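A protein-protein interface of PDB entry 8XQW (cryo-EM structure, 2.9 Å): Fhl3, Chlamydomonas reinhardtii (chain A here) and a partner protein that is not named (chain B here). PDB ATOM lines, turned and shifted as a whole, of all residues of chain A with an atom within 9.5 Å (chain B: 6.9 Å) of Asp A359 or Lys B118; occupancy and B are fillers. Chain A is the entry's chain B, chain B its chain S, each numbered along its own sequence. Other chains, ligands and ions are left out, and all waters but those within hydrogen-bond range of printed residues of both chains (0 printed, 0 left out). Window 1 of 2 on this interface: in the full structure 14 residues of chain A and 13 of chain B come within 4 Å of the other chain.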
ATOM      1  N   GLU A 254       3.873 -17.952 -39.567  1.00  0.00           N
ATOM      2  CA  GLU A 254       3.753 -17.232 -38.308  1.00  0.00           C
ATOM      3  C   GLU A 254       3.676 -18.163 -37.108  1.00  0.00           C
ATOM      4  O   GLU A 254       3.059 -17.817 -36.099  1.00  0.00           O
ATOM      5  CB  GLU A 254       2.541 -16.308 -38.335  1.00  0.00           C
ATOM      6  CG  GLU A 254       1.234 -17.008 -38.564  1.00  0.00           C
ATOM      7  CD  GLU A 254       0.132 -16.042 -38.939  1.00  0.00           C
ATOM      8  OE1 GLU A 254      -0.994 -16.189 -38.420  1.00  0.00           O
ATOM      9  OE2 GLU A 254       0.393 -15.132 -39.750  1.00  0.00           O
ATOM     10  N   VAL A 255       4.279 -19.342 -37.196  1.00  0.00           N
ATOM     11  CA  VAL A 255       4.379 -20.235 -36.048  1.00  0.00           C
ATOM     12  C   VAL A 255       5.785 -20.113 -35.480  1.00  0.00           C
ATOM     13  O   VAL A 255       6.751 -20.525 -36.135  1.00  0.00           O
ATOM     14  CB  VAL A 255       4.050 -21.682 -36.437  1.00  0.00           C
ATOM     15  CG1 VAL A 255       4.280 -22.599 -35.269  1.00  0.00           C
ATOM     16  CG2 VAL A 255       2.626 -21.783 -36.893  1.00  0.00           C
ATOM     17  N   PRO A 256       5.952 -19.564 -34.286  1.00  0.00           N
ATOM     18  CA  PRO A 256       7.292 -19.348 -33.746  1.00  0.00           C
ATOM     19  C   PRO A 256       7.855 -20.615 -33.122  1.00  0.00           C
ATOM     20  O   PRO A 256       7.131 -21.471 -32.623  1.00  0.00           O
ATOM     21  CB  PRO A 256       7.056 -18.281 -32.686  1.00  0.00           C
ATOM     22  CG  PRO A 256       5.701 -18.580 -32.201  1.00  0.00           C
ATOM     23  CD  PRO A 256       4.917 -19.034 -33.389  1.00  0.00           C
ATOM     24  N   ASN A 257       9.178 -20.705 -33.146  1.00  0.00           N
ATOM     25  CA  ASN A 257       9.872 -21.847 -32.575  1.00  0.00           C
ATOM     26  C   ASN A 257       9.691 -21.885 -31.064  1.00  0.00           C
ATOM     27  O   ASN A 257       9.559 -20.849 -30.413  1.00  0.00           O
ATOM     28  CB  ASN A 257      11.355 -21.782 -32.917  1.00  0.00           C
ATOM     29  CG  ASN A 257      12.132 -22.954 -32.370  1.00  0.00           C
ATOM     30  OD1 ASN A 257      12.303 -23.966 -33.041  1.00  0.00           O
ATOM     31  ND2 ASN A 257      12.623 -22.820 -31.152  1.00  0.00           N
ATOM     32  N   ARG A 258       9.666 -23.094 -30.513  1.00  0.00           N
ATOM     33  CA  ARG A 258       9.669 -23.304 -29.074  1.00  0.00           C
ATOM     34  C   ARG A 258      10.499 -24.538 -28.789  1.00  0.00           C
ATOM     35  O   ARG A 258      10.234 -25.605 -29.344  1.00  0.00           O
ATOM     36  CB  ARG A 258       8.258 -23.483 -28.515  1.00  0.00           C
ATOM     37  CG  ARG A 258       7.338 -22.303 -28.705  1.00  0.00           C
ATOM     38  CD  ARG A 258       7.339 -21.409 -27.498  1.00  0.00           C
ATOM     39  NE  ARG A 258       6.486 -20.240 -27.667  1.00  0.00           N
ATOM     40  CZ  ARG A 258       6.768 -19.211 -28.457  1.00  0.00           C
ATOM     41  NH1 ARG A 258       7.881 -19.201 -29.166  1.00  0.00           N
ATOM     42  NH2 ARG A 258       5.938 -18.189 -28.531  1.00  0.00           N
ATOM     43  N   ASN A 259      11.495 -24.398 -27.926  1.00  0.00           N
ATOM     44  CA  ASN A 259      12.441 -25.469 -27.667  1.00  0.00           C
ATOM     45  C   ASN A 259      11.986 -26.309 -26.485  1.00  0.00           C
ATOM     46  O   ASN A 259      11.404 -25.794 -25.530  1.00  0.00           O
ATOM     47  CB  ASN A 259      13.829 -24.898 -27.390  1.00  0.00           C
ATOM     48  CG  ASN A 259      14.333 -24.016 -28.510  1.00  0.00           C
ATOM     49  OD1 ASN A 259      14.016 -22.835 -28.577  1.00  0.00           O
ATOM     50  ND2 ASN A 259      15.135 -24.587 -29.392  1.00  0.00           N
ATOM     51  N   SER A 260      12.253 -27.608 -26.559  1.00  0.00           N
ATOM     52  CA  SER A 260      12.054 -28.483 -25.418  1.00  0.00           C
ATOM     53  C   SER A 260      13.224 -28.329 -24.454  1.00  0.00           C
ATOM     54  O   SER A 260      14.035 -27.412 -24.566  1.00  0.00           O
ATOM     55  CB  SER A 260      11.908 -29.928 -25.875  1.00  0.00           C
ATOM     56  OG  SER A 260      12.944 -30.282 -26.764  1.00  0.00           O
ATOM     57  N   ARG A 261      13.326 -29.240 -23.491  1.00  0.00           N
ATOM     58  CA  ARG A 261      14.403 -29.119 -22.516  1.00  0.00           C
ATOM     59  C   ARG A 261      15.749 -29.501 -23.119  1.00  0.00           C
ATOM     60  O   ARG A 261      16.763 -28.850 -22.844  1.00  0.00           O
ATOM     61  CB  ARG A 261      14.102 -29.972 -21.289  1.00  0.00           C
ATOM     62  CG  ARG A 261      12.805 -29.623 -20.596  1.00  0.00           C
ATOM     63  CD  ARG A 261      12.551 -28.132 -20.594  1.00  0.00           C
ATOM     64  NE  ARG A 261      13.440 -27.428 -19.683  1.00  0.00           N
ATOM     65  CZ  ARG A 261      13.429 -26.113 -19.500  1.00  0.00           C
ATOM     66  NH1 ARG A 261      12.572 -25.356 -20.168  1.00  0.00           N
ATOM     67  NH2 ARG A 261      14.277 -25.554 -18.651  1.00  0.00           N
ATOM     68  N   VAL A 264      16.987 -26.658 -25.047  1.00  0.00           N
ATOM     69  CA  VAL A 264      17.471 -25.614 -24.150  1.00  0.00           C
ATOM     70  C   VAL A 264      18.889 -25.925 -23.688  1.00  0.00           C
ATOM     71  O   VAL A 264      19.750 -25.038 -23.632  1.00  0.00           O
ATOM     72  CB  VAL A 264      16.514 -25.452 -22.958  1.00  0.00           C
ATOM     73  CG1 VAL A 264      17.188 -24.678 -21.851  1.00  0.00           C
ATOM     74  CG2 VAL A 264      15.254 -24.755 -23.386  1.00  0.00           C
ATOM     75  N   ALA A 353      20.183 -14.399 -20.990  1.00  0.00           N
ATOM     76  CA  ALA A 353      18.927 -14.019 -20.353  1.00  0.00           C
ATOM     77  C   ALA A 353      17.739 -14.634 -21.070  1.00  0.00           C
ATOM     78  O   ALA A 353      16.803 -15.117 -20.423  1.00  0.00           O
ATOM     79  CB  ALA A 353      18.790 -12.500 -20.315  1.00  0.00           C
ATOM     80  N   MET A 354      17.788 -14.624 -22.398  1.00  0.00           N
ATOM     81  CA  MET A 354      16.653 -15.135 -23.204  1.00  0.00           C
ATOM     82  C   MET A 354      16.680 -16.667 -23.254  1.00  0.00           C
ATOM     83  O   MET A 354      15.618 -17.257 -23.504  1.00  0.00           O
ATOM     84  CB  MET A 354      16.702 -14.555 -24.618  1.00  0.00           C
ATOM     85  CG  MET A 354      16.290 -13.106 -24.653  1.00  0.00           C
ATOM     86  SD  MET A 354      16.198 -12.524 -26.353  1.00  0.00           S
ATOM     87  CE  MET A 354      16.396 -14.109 -27.174  1.00  0.00           C
ATOM     88  N   ALA A 355      17.833 -17.286 -23.014  1.00  0.00           N
ATOM     89  CA  ALA A 355      17.897 -18.765 -22.968  1.00  0.00           C
ATOM     90  C   ALA A 355      17.658 -19.237 -21.540  1.00  0.00           C
ATOM     91  O   ALA A 355      18.282 -20.227 -21.134  1.00  0.00           O
ATOM     92  CB  ALA A 355      19.230 -19.253 -23.472  1.00  0.00           C
ATOM     93  N   LEU A 356      16.779 -18.552 -20.816  1.00  0.00           N
ATOM     94  CA  LEU A 356      16.441 -18.981 -19.441  1.00  0.00           C
ATOM     95  C   LEU A 356      15.026 -18.507 -19.109  1.00  0.00           C
ATOM     96  O   LEU A 356      14.240 -19.317 -18.591  1.00  0.00           O
ATOM     97  CB  LEU A 356      17.460 -18.381 -18.484  1.00  0.00           C
ATOM     98  CG  LEU A 356      18.219 -19.367 -17.594  1.00  0.00           C
ATOM     99  CD1 LEU A 356      19.319 -18.645 -16.839  1.00  0.00           C
ATOM    100  CD2 LEU A 356      17.266 -20.035 -16.621  1.00  0.00           C
ATOM    101  N   PHE A 357      14.720 -17.242 -19.385  1.00  0.00           N
ATOM    102  CA  PHE A 357      13.386 -16.694 -19.033  1.00  0.00           C
ATOM    103  C   PHE A 357      12.745 -16.188 -20.298  1.00  0.00           C
ATOM    104  O   PHE A 357      11.818 -15.364 -20.232  1.00  0.00           O
ATOM    105  CB  PHE A 357      13.532 -15.576 -18.001  1.00  0.00           C
ATOM    106  CG  PHE A 357      14.739 -15.703 -17.081  1.00  0.00           C
ATOM    107  CD1 PHE A 357      14.717 -16.564 -15.992  1.00  0.00           C
ATOM    108  CD2 PHE A 357      15.890 -14.959 -17.308  1.00  0.00           C
ATOM    109  CE1 PHE A 357      15.816 -16.678 -15.158  1.00  0.00           C
ATOM    110  CE2 PHE A 357      16.987 -15.081 -16.473  1.00  0.00           C
ATOM    111  CZ  PHE A 357      16.947 -15.938 -15.400  1.00  0.00           C
ATOM    112  N   GLY A 358      13.208 -16.688 -21.438  1.00  0.00           N
ATOM    113  CA  GLY A 358      12.698 -16.167 -22.714  1.00  0.00           C
ATOM    114  C   GLY A 358      11.509 -16.947 -23.201  1.00  0.00           C
ATOM    115  O   GLY A 358      11.417 -18.136 -22.864  1.00  0.00           O
ATOM    116  N   ASP A 359      10.676 -16.333 -24.039  1.00  0.00           N
ATOM    117  CA  ASP A 359       9.425 -16.995 -24.483  1.00  0.00           C
ATOM    118  C   ASP A 359       9.753 -18.328 -25.147  1.00  0.00           C
ATOM    119  O   ASP A 359       9.098 -19.316 -24.786  1.00  0.00           O
ATOM    120  CB  ASP A 359       8.610 -16.080 -25.370  1.00  0.00           C
ATOM    121  CG  ASP A 359       7.622 -15.191 -24.628  1.00  0.00           C
ATOM    122  OD1 ASP A 359       7.774 -15.053 -23.397  1.00  0.00           O
ATOM    123  OD2 ASP A 359       6.711 -14.649 -25.287  1.00  0.00           O
ATOM    124  N   ALA A 360      10.738 -18.381 -26.040  1.00  0.00           N
ATOM    125  CA  ALA A 360      10.983 -19.650 -26.759  1.00  0.00           C
ATOM    126  C   ALA A 360      11.439 -20.743 -25.802  1.00  0.00           C
ATOM    127  O   ALA A 360      11.475 -21.902 -26.230  1.00  0.00           O
ATOM    128  CB  ALA A 360      12.005 -19.452 -27.821  1.00  0.00           C
ATOM    129  N   ASN A 361      11.789 -20.410 -24.567  1.00  0.00           N
ATOM    130  CA  ASN A 361      12.341 -21.443 -23.657  1.00  0.00           C
ATOM    131  C   ASN A 361      11.538 -21.461 -22.358  1.00  0.00           C
ATOM    132  O   ASN A 361      12.078 -21.922 -21.348  1.00  0.00           O
ATOM    133  CB  ASN A 361      13.823 -21.209 -23.415  1.00  0.00           C
ATOM    134  CG  ASN A 361      14.606 -20.991 -24.684  1.00  0.00           C
ATOM    135  OD1 ASN A 361      15.048 -21.953 -25.317  1.00  0.00           O
ATOM    136  ND2 ASN A 361      14.807 -19.738 -25.063  1.00  0.00           N
ATOM    137  N   SER A 362      10.286 -21.015 -22.389  1.00  0.00           N
ATOM    138  CA  SER A 362       9.483 -20.923 -21.184  1.00  0.00           C
ATOM    139  C   SER A 362       8.320 -21.896 -21.136  1.00  0.00           C
ATOM    140  O   SER A 362       7.574 -21.887 -20.152  1.00  0.00           O
ATOM    141  CB  SER A 362       8.937 -19.500 -21.017  1.00  0.00           C
ATOM    142  OG  SER A 362       9.985 -18.553 -21.059  1.00  0.00           O
ATOM    143  N   VAL A 363       8.133 -22.722 -22.159  1.00  0.00           N
ATOM    144  CA  VAL A 363       7.081 -23.730 -22.162  1.00  0.00           C
ATOM    145  C   VAL A 363       7.750 -25.068 -21.887  1.00  0.00           C
ATOM    146  O   VAL A 363       8.412 -25.630 -22.759  1.00  0.00           O
ATOM    147  CB  VAL A 363       6.321 -23.743 -23.491  1.00  0.00           C
ATOM    148  CG1 VAL A 363       4.953 -24.321 -23.301  1.00  0.00           C
ATOM    149  CG2 VAL A 363       6.217 -22.345 -24.045  1.00  0.00           C
ATOM    150  N   LYS A 364       7.585 -25.579 -20.669  1.00  0.00           N
ATOM    151  CA  LYS A 364       8.329 -26.759 -20.253  1.00  0.00           C
ATOM    152  C   LYS A 364       7.850 -28.038 -20.921  1.00  0.00           C
ATOM    153  O   LYS A 364       8.591 -29.025 -20.925  1.00  0.00           O
ATOM    154  CB  LYS A 364       8.243 -26.915 -18.742  1.00  0.00           C
ATOM    155  CG  LYS A 364       9.171 -25.999 -17.985  1.00  0.00           C
ATOM    156  CD  LYS A 364       9.520 -26.595 -16.641  1.00  0.00           C
ATOM    157  CE  LYS A 364      10.706 -25.893 -16.023  1.00  0.00           C
ATOM    158  NZ  LYS A 364      11.412 -26.785 -15.068  1.00  0.00           N
ATOM    159  N   ALA A 366       6.876 -28.445 -24.268  1.00  0.00           N
ATOM    160  CA  ALA A 366       6.835 -28.232 -25.707  1.00  0.00           C
ATOM    161  C   ALA A 366       7.654 -29.332 -26.355  1.00  0.00           C
ATOM    162  O   ALA A 366       8.836 -29.484 -26.049  1.00  0.00           O
ATOM    163  CB  ALA A 366       7.383 -26.857 -26.064  1.00  0.00           C
ATOM    164  N   THR A 369       7.049 -28.108 -31.908  1.00  0.00           N
ATOM    165  CA  THR A 369       5.873 -27.322 -32.241  1.00  0.00           C
ATOM    166  C   THR A 369       5.883 -26.869 -33.689  1.00  0.00           C
ATOM    167  O   THR A 369       4.847 -26.894 -34.352  1.00  0.00           O
ATOM    168  CB  THR A 369       5.761 -26.116 -31.318  1.00  0.00           C
ATOM    169  OG1 THR A 369       6.778 -25.174 -31.654  1.00  0.00           O
ATOM    170  CG2 THR A 369       5.932 -26.544 -29.887  1.00  0.00           C
ATOM    171  N   SER B 102      12.340  -8.263 -31.383  1.00  0.00           N
ATOM    172  CA  SER B 102      11.620  -9.456 -30.956  1.00  0.00           C
ATOM    173  C   SER B 102      11.151  -9.343 -29.515  1.00  0.00           C
ATOM    174  O   SER B 102       9.973  -9.576 -29.219  1.00  0.00           O
ATOM    175  CB  SER B 102      12.505 -10.686 -31.123  1.00  0.00           C
ATOM    176  OG  SER B 102      12.305 -11.591 -30.053  1.00  0.00           O
ATOM    177  N   VAL B 103      12.046  -8.984 -28.601  1.00  0.00           N
ATOM    178  CA  VAL B 103      11.684  -9.009 -27.187  1.00  0.00           C
ATOM    179  C   VAL B 103      10.824  -7.815 -26.802  1.00  0.00           C
ATOM    180  O   VAL B 103       9.663  -7.973 -26.421  1.00  0.00           O
ATOM    181  CB  VAL B 103      12.951  -9.086 -26.318  1.00  0.00           C
ATOM    182  CG1 VAL B 103      12.567  -9.169 -24.857  1.00  0.00           C
ATOM    183  CG2 VAL B 103      13.772 -10.287 -26.712  1.00  0.00           C
ATOM    184  N   ASP B 113       1.261  -3.079 -28.534  1.00  0.00           N
ATOM    185  CA  ASP B 113       1.315  -3.445 -29.942  1.00  0.00           C
ATOM    186  C   ASP B 113       2.031  -4.774 -30.131  1.00  0.00           C
ATOM    187  O   ASP B 113       1.668  -5.561 -31.010  1.00  0.00           O
ATOM    188  CB  ASP B 113       1.982  -2.333 -30.740  1.00  0.00           C
ATOM    189  CG  ASP B 113       1.412  -0.973 -30.408  1.00  0.00           C
ATOM    190  OD1 ASP B 113       0.744  -0.860 -29.361  1.00  0.00           O
ATOM    191  OD2 ASP B 113       1.626  -0.023 -31.190  1.00  0.00           O
ATOM    192  N   VAL B 114       3.010  -5.072 -29.279  1.00  0.00           N
ATOM    193  CA  VAL B 114       3.623  -6.395 -29.309  1.00  0.00           C
ATOM    194  C   VAL B 114       2.622  -7.454 -28.872  1.00  0.00           C
ATOM    195  O   VAL B 114       2.563  -8.549 -29.447  1.00  0.00           O
ATOM    196  CB  VAL B 114       4.891  -6.419 -28.439  1.00  0.00           C
ATOM    197  CG1 VAL B 114       5.274  -7.841 -28.100  1.00  0.00           C
ATOM    198  CG2 VAL B 114       6.018  -5.750 -29.174  1.00  0.00           C
ATOM    199  N   ALA B 115       1.816  -7.152 -27.852  1.00  0.00           N
ATOM    200  CA  ALA B 115       0.824  -8.120 -27.395  1.00  0.00           C
ATOM    201  C   ALA B 115      -0.192  -8.424 -28.484  1.00  0.00           C
ATOM    202  O   ALA B 115      -0.544  -9.585 -28.705  1.00  0.00           O
ATOM    203  CB  ALA B 115       0.121  -7.612 -26.141  1.00  0.00           C
ATOM    204  N   VAL B 116      -0.670  -7.396 -29.183  1.00  0.00           N
ATOM    205  CA  VAL B 116      -1.631  -7.635 -30.255  1.00  0.00           C
ATOM    206  C   VAL B 116      -0.941  -8.225 -31.479  1.00  0.00           C
ATOM    207  O   VAL B 116      -1.598  -8.776 -32.366  1.00  0.00           O
ATOM    208  CB  VAL B 116      -2.391  -6.345 -30.606  1.00  0.00           C
ATOM    209  CG1 VAL B 116      -2.920  -5.689 -29.356  1.00  0.00           C
ATOM    210  CG2 VAL B 116      -1.503  -5.399 -31.380  1.00  0.00           C
ATOM    211  N   ARG B 117       0.383  -8.111 -31.559  1.00  0.00           N
ATOM    212  CA  ARG B 117       1.088  -8.761 -32.655  1.00  0.00           C
ATOM    213  C   ARG B 117       1.216 -10.257 -32.419  1.00  0.00           C
ATOM    214  O   ARG B 117       0.983 -11.053 -33.333  1.00  0.00           O
ATOM    215  CB  ARG B 117       2.466  -8.131 -32.845  1.00  0.00           C
ATOM    216  CG  ARG B 117       3.241  -8.685 -34.023  1.00  0.00           C
ATOM    217  CD  ARG B 117       4.545  -9.315 -33.580  1.00  0.00           C
ATOM    218  NE  ARG B 117       5.358  -8.391 -32.795  1.00  0.00           N
ATOM    219  CZ  ARG B 117       6.483  -8.728 -32.170  1.00  0.00           C
ATOM    220  NH1 ARG B 117       6.941  -9.969 -32.244  1.00  0.00           N
ATOM    221  NH2 ARG B 117       7.156  -7.819 -31.476  1.00  0.00           N
ATOM    222  N   LYS B 118       1.587 -10.663 -31.211  1.00  0.00           N
ATOM    223  CA  LYS B 118       1.809 -12.077 -30.943  1.00  0.00           C
ATOM    224  C   LYS B 118       0.564 -12.795 -30.439  1.00  0.00           C
ATOM    225  O   LYS B 118       0.634 -13.992 -30.153  1.00  0.00           O
ATOM    226  CB  LYS B 118       2.954 -12.258 -29.945  1.00  0.00           C
ATOM    227  CG  LYS B 118       2.734 -11.611 -28.605  1.00  0.00           C
ATOM    228  CD  LYS B 118       3.718 -12.142 -27.581  1.00  0.00           C
ATOM    229  CE  LYS B 118       5.139 -12.099 -28.097  1.00  0.00           C
ATOM    230  NZ  LYS B 118       6.068 -12.778 -27.159  1.00  0.00           N
ATOM    231  N   LEU B 119      -0.563 -12.103 -30.319  1.00  0.00           N
ATOM    232  CA  LEU B 119      -1.846 -12.742 -30.071  1.00  0.00           C
ATOM    233  C   LEU B 119      -2.693 -12.834 -31.326  1.00  0.00           C
ATOM    234  O   LEU B 119      -3.791 -13.392 -31.277  1.00  0.00           O
ATOM    235  CB  LEU B 119      -2.623 -11.985 -28.993  1.00  0.00           C
ATOM    236  CG  LEU B 119      -2.489 -12.480 -27.560  1.00  0.00           C
ATOM    237  CD1 LEU B 119      -3.393 -11.689 -26.646  1.00  0.00           C
ATOM    238  CD2 LEU B 119      -2.828 -13.945 -27.503  1.00  0.00           C
ATOM    239  N   ARG B 120      -2.212 -12.284 -32.441  1.00  0.00           N
ATOM    240  CA  ARG B 120      -2.922 -12.310 -33.718  1.00  0.00           C
ATOM    241  C   ARG B 120      -4.359 -11.821 -33.563  1.00  0.00           C
ATOM    242  O   ARG B 120      -5.307 -12.451 -34.035  1.00  0.00           O
ATOM    243  CB  ARG B 120      -2.878 -13.703 -34.341  1.00  0.00           C
ATOM    244  CG  ARG B 120      -1.498 -14.122 -34.804  1.00  0.00           C
ATOM    245  CD  ARG B 120      -1.493 -15.551 -35.308  1.00  0.00           C
ATOM    246  NE  ARG B 120      -2.291 -15.707 -36.518  1.00  0.00           N
ATOM    247  CZ  ARG B 120      -3.486 -16.285 -36.553  1.00  0.00           C
ATOM    248  NH1 ARG B 120      -4.022 -16.766 -35.441  1.00  0.00           N
ATOM    249  NH2 ARG B 120      -4.146 -16.382 -37.698  1.00  0.00           N
ATOM    250  N   LEU B 121      -4.518 -10.685 -32.893  1.00  0.00           N
ATOM    251  CA  LEU B 121      -5.838 -10.103 -32.712  1.00  0.00           C
ATOM    252  C   LEU B 121      -6.286  -9.261 -33.894  1.00  0.00           C
ATOM    253  O   LEU B 121      -7.489  -9.033 -34.050  1.00  0.00           O
ATOM    254  CB  LEU B 121      -5.874  -9.236 -31.456  1.00  0.00           C
ATOM    255  CG  LEU B 121      -5.738  -9.970 -30.132  1.00  0.00           C
ATOM    256  CD1 LEU B 121      -6.258  -9.093 -29.013  1.00  0.00           C
ATOM    257  CD2 LEU B 121      -6.488 -11.280 -30.189  1.00  0.00           C
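Asp A359 touches one residue of chain B. Lys B118 touches just one residue of chain A: Asp A359 (2.7 Å). No residue of chain A comes within 4 Å of Ala B115. Of the printed residues of chain B, Met A354 touches Val B103 (3.3 Å). Of the printed residues of chain A, Val B103 touches Met A354. Printed residues of chain B within 4 Å of Glu A254: Arg B120 (2.4 Å). Of the printed residues of chain A, Arg B120 touches Glu A254. The nearest printed residue of chain B that does not touch Asp A359 is Ser B102 (7.2 Å). The nearest residue of chain A that does not touch Lys B118 is Arg A258 (5.6 Å). The nearest printed residue of chain A that does not touch Arg B120 is Val A255 (7.2 Å).
The backbone carbonyl oxygen (O) of Met A354 is in hydrogen-bond range of the side-chain amide nitrogen (ND2) of Asn A361 (3.0 Å).
Printed residues of chain B that touch a printed residue of chain A: Val B103, Lys B118 and Arg B120. Hydrophobic or aromatic side chains of chain B within 4 Å of the printed part of chain A: Val B103. Printed residues of chain A that touch a printed residue of chain B: Glu A254, Met A354 and Asp A359.
Met A354 touches Val B103.
The guanidinium group (NH2) of Arg B120 is in salt-bridge range of the side-chain carboxylate (OE1) of Glu A254 (3.2 Å). NZ of Lys B118 is in salt-bridge range of OD2 of Asp A359, 2.7 Å away.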
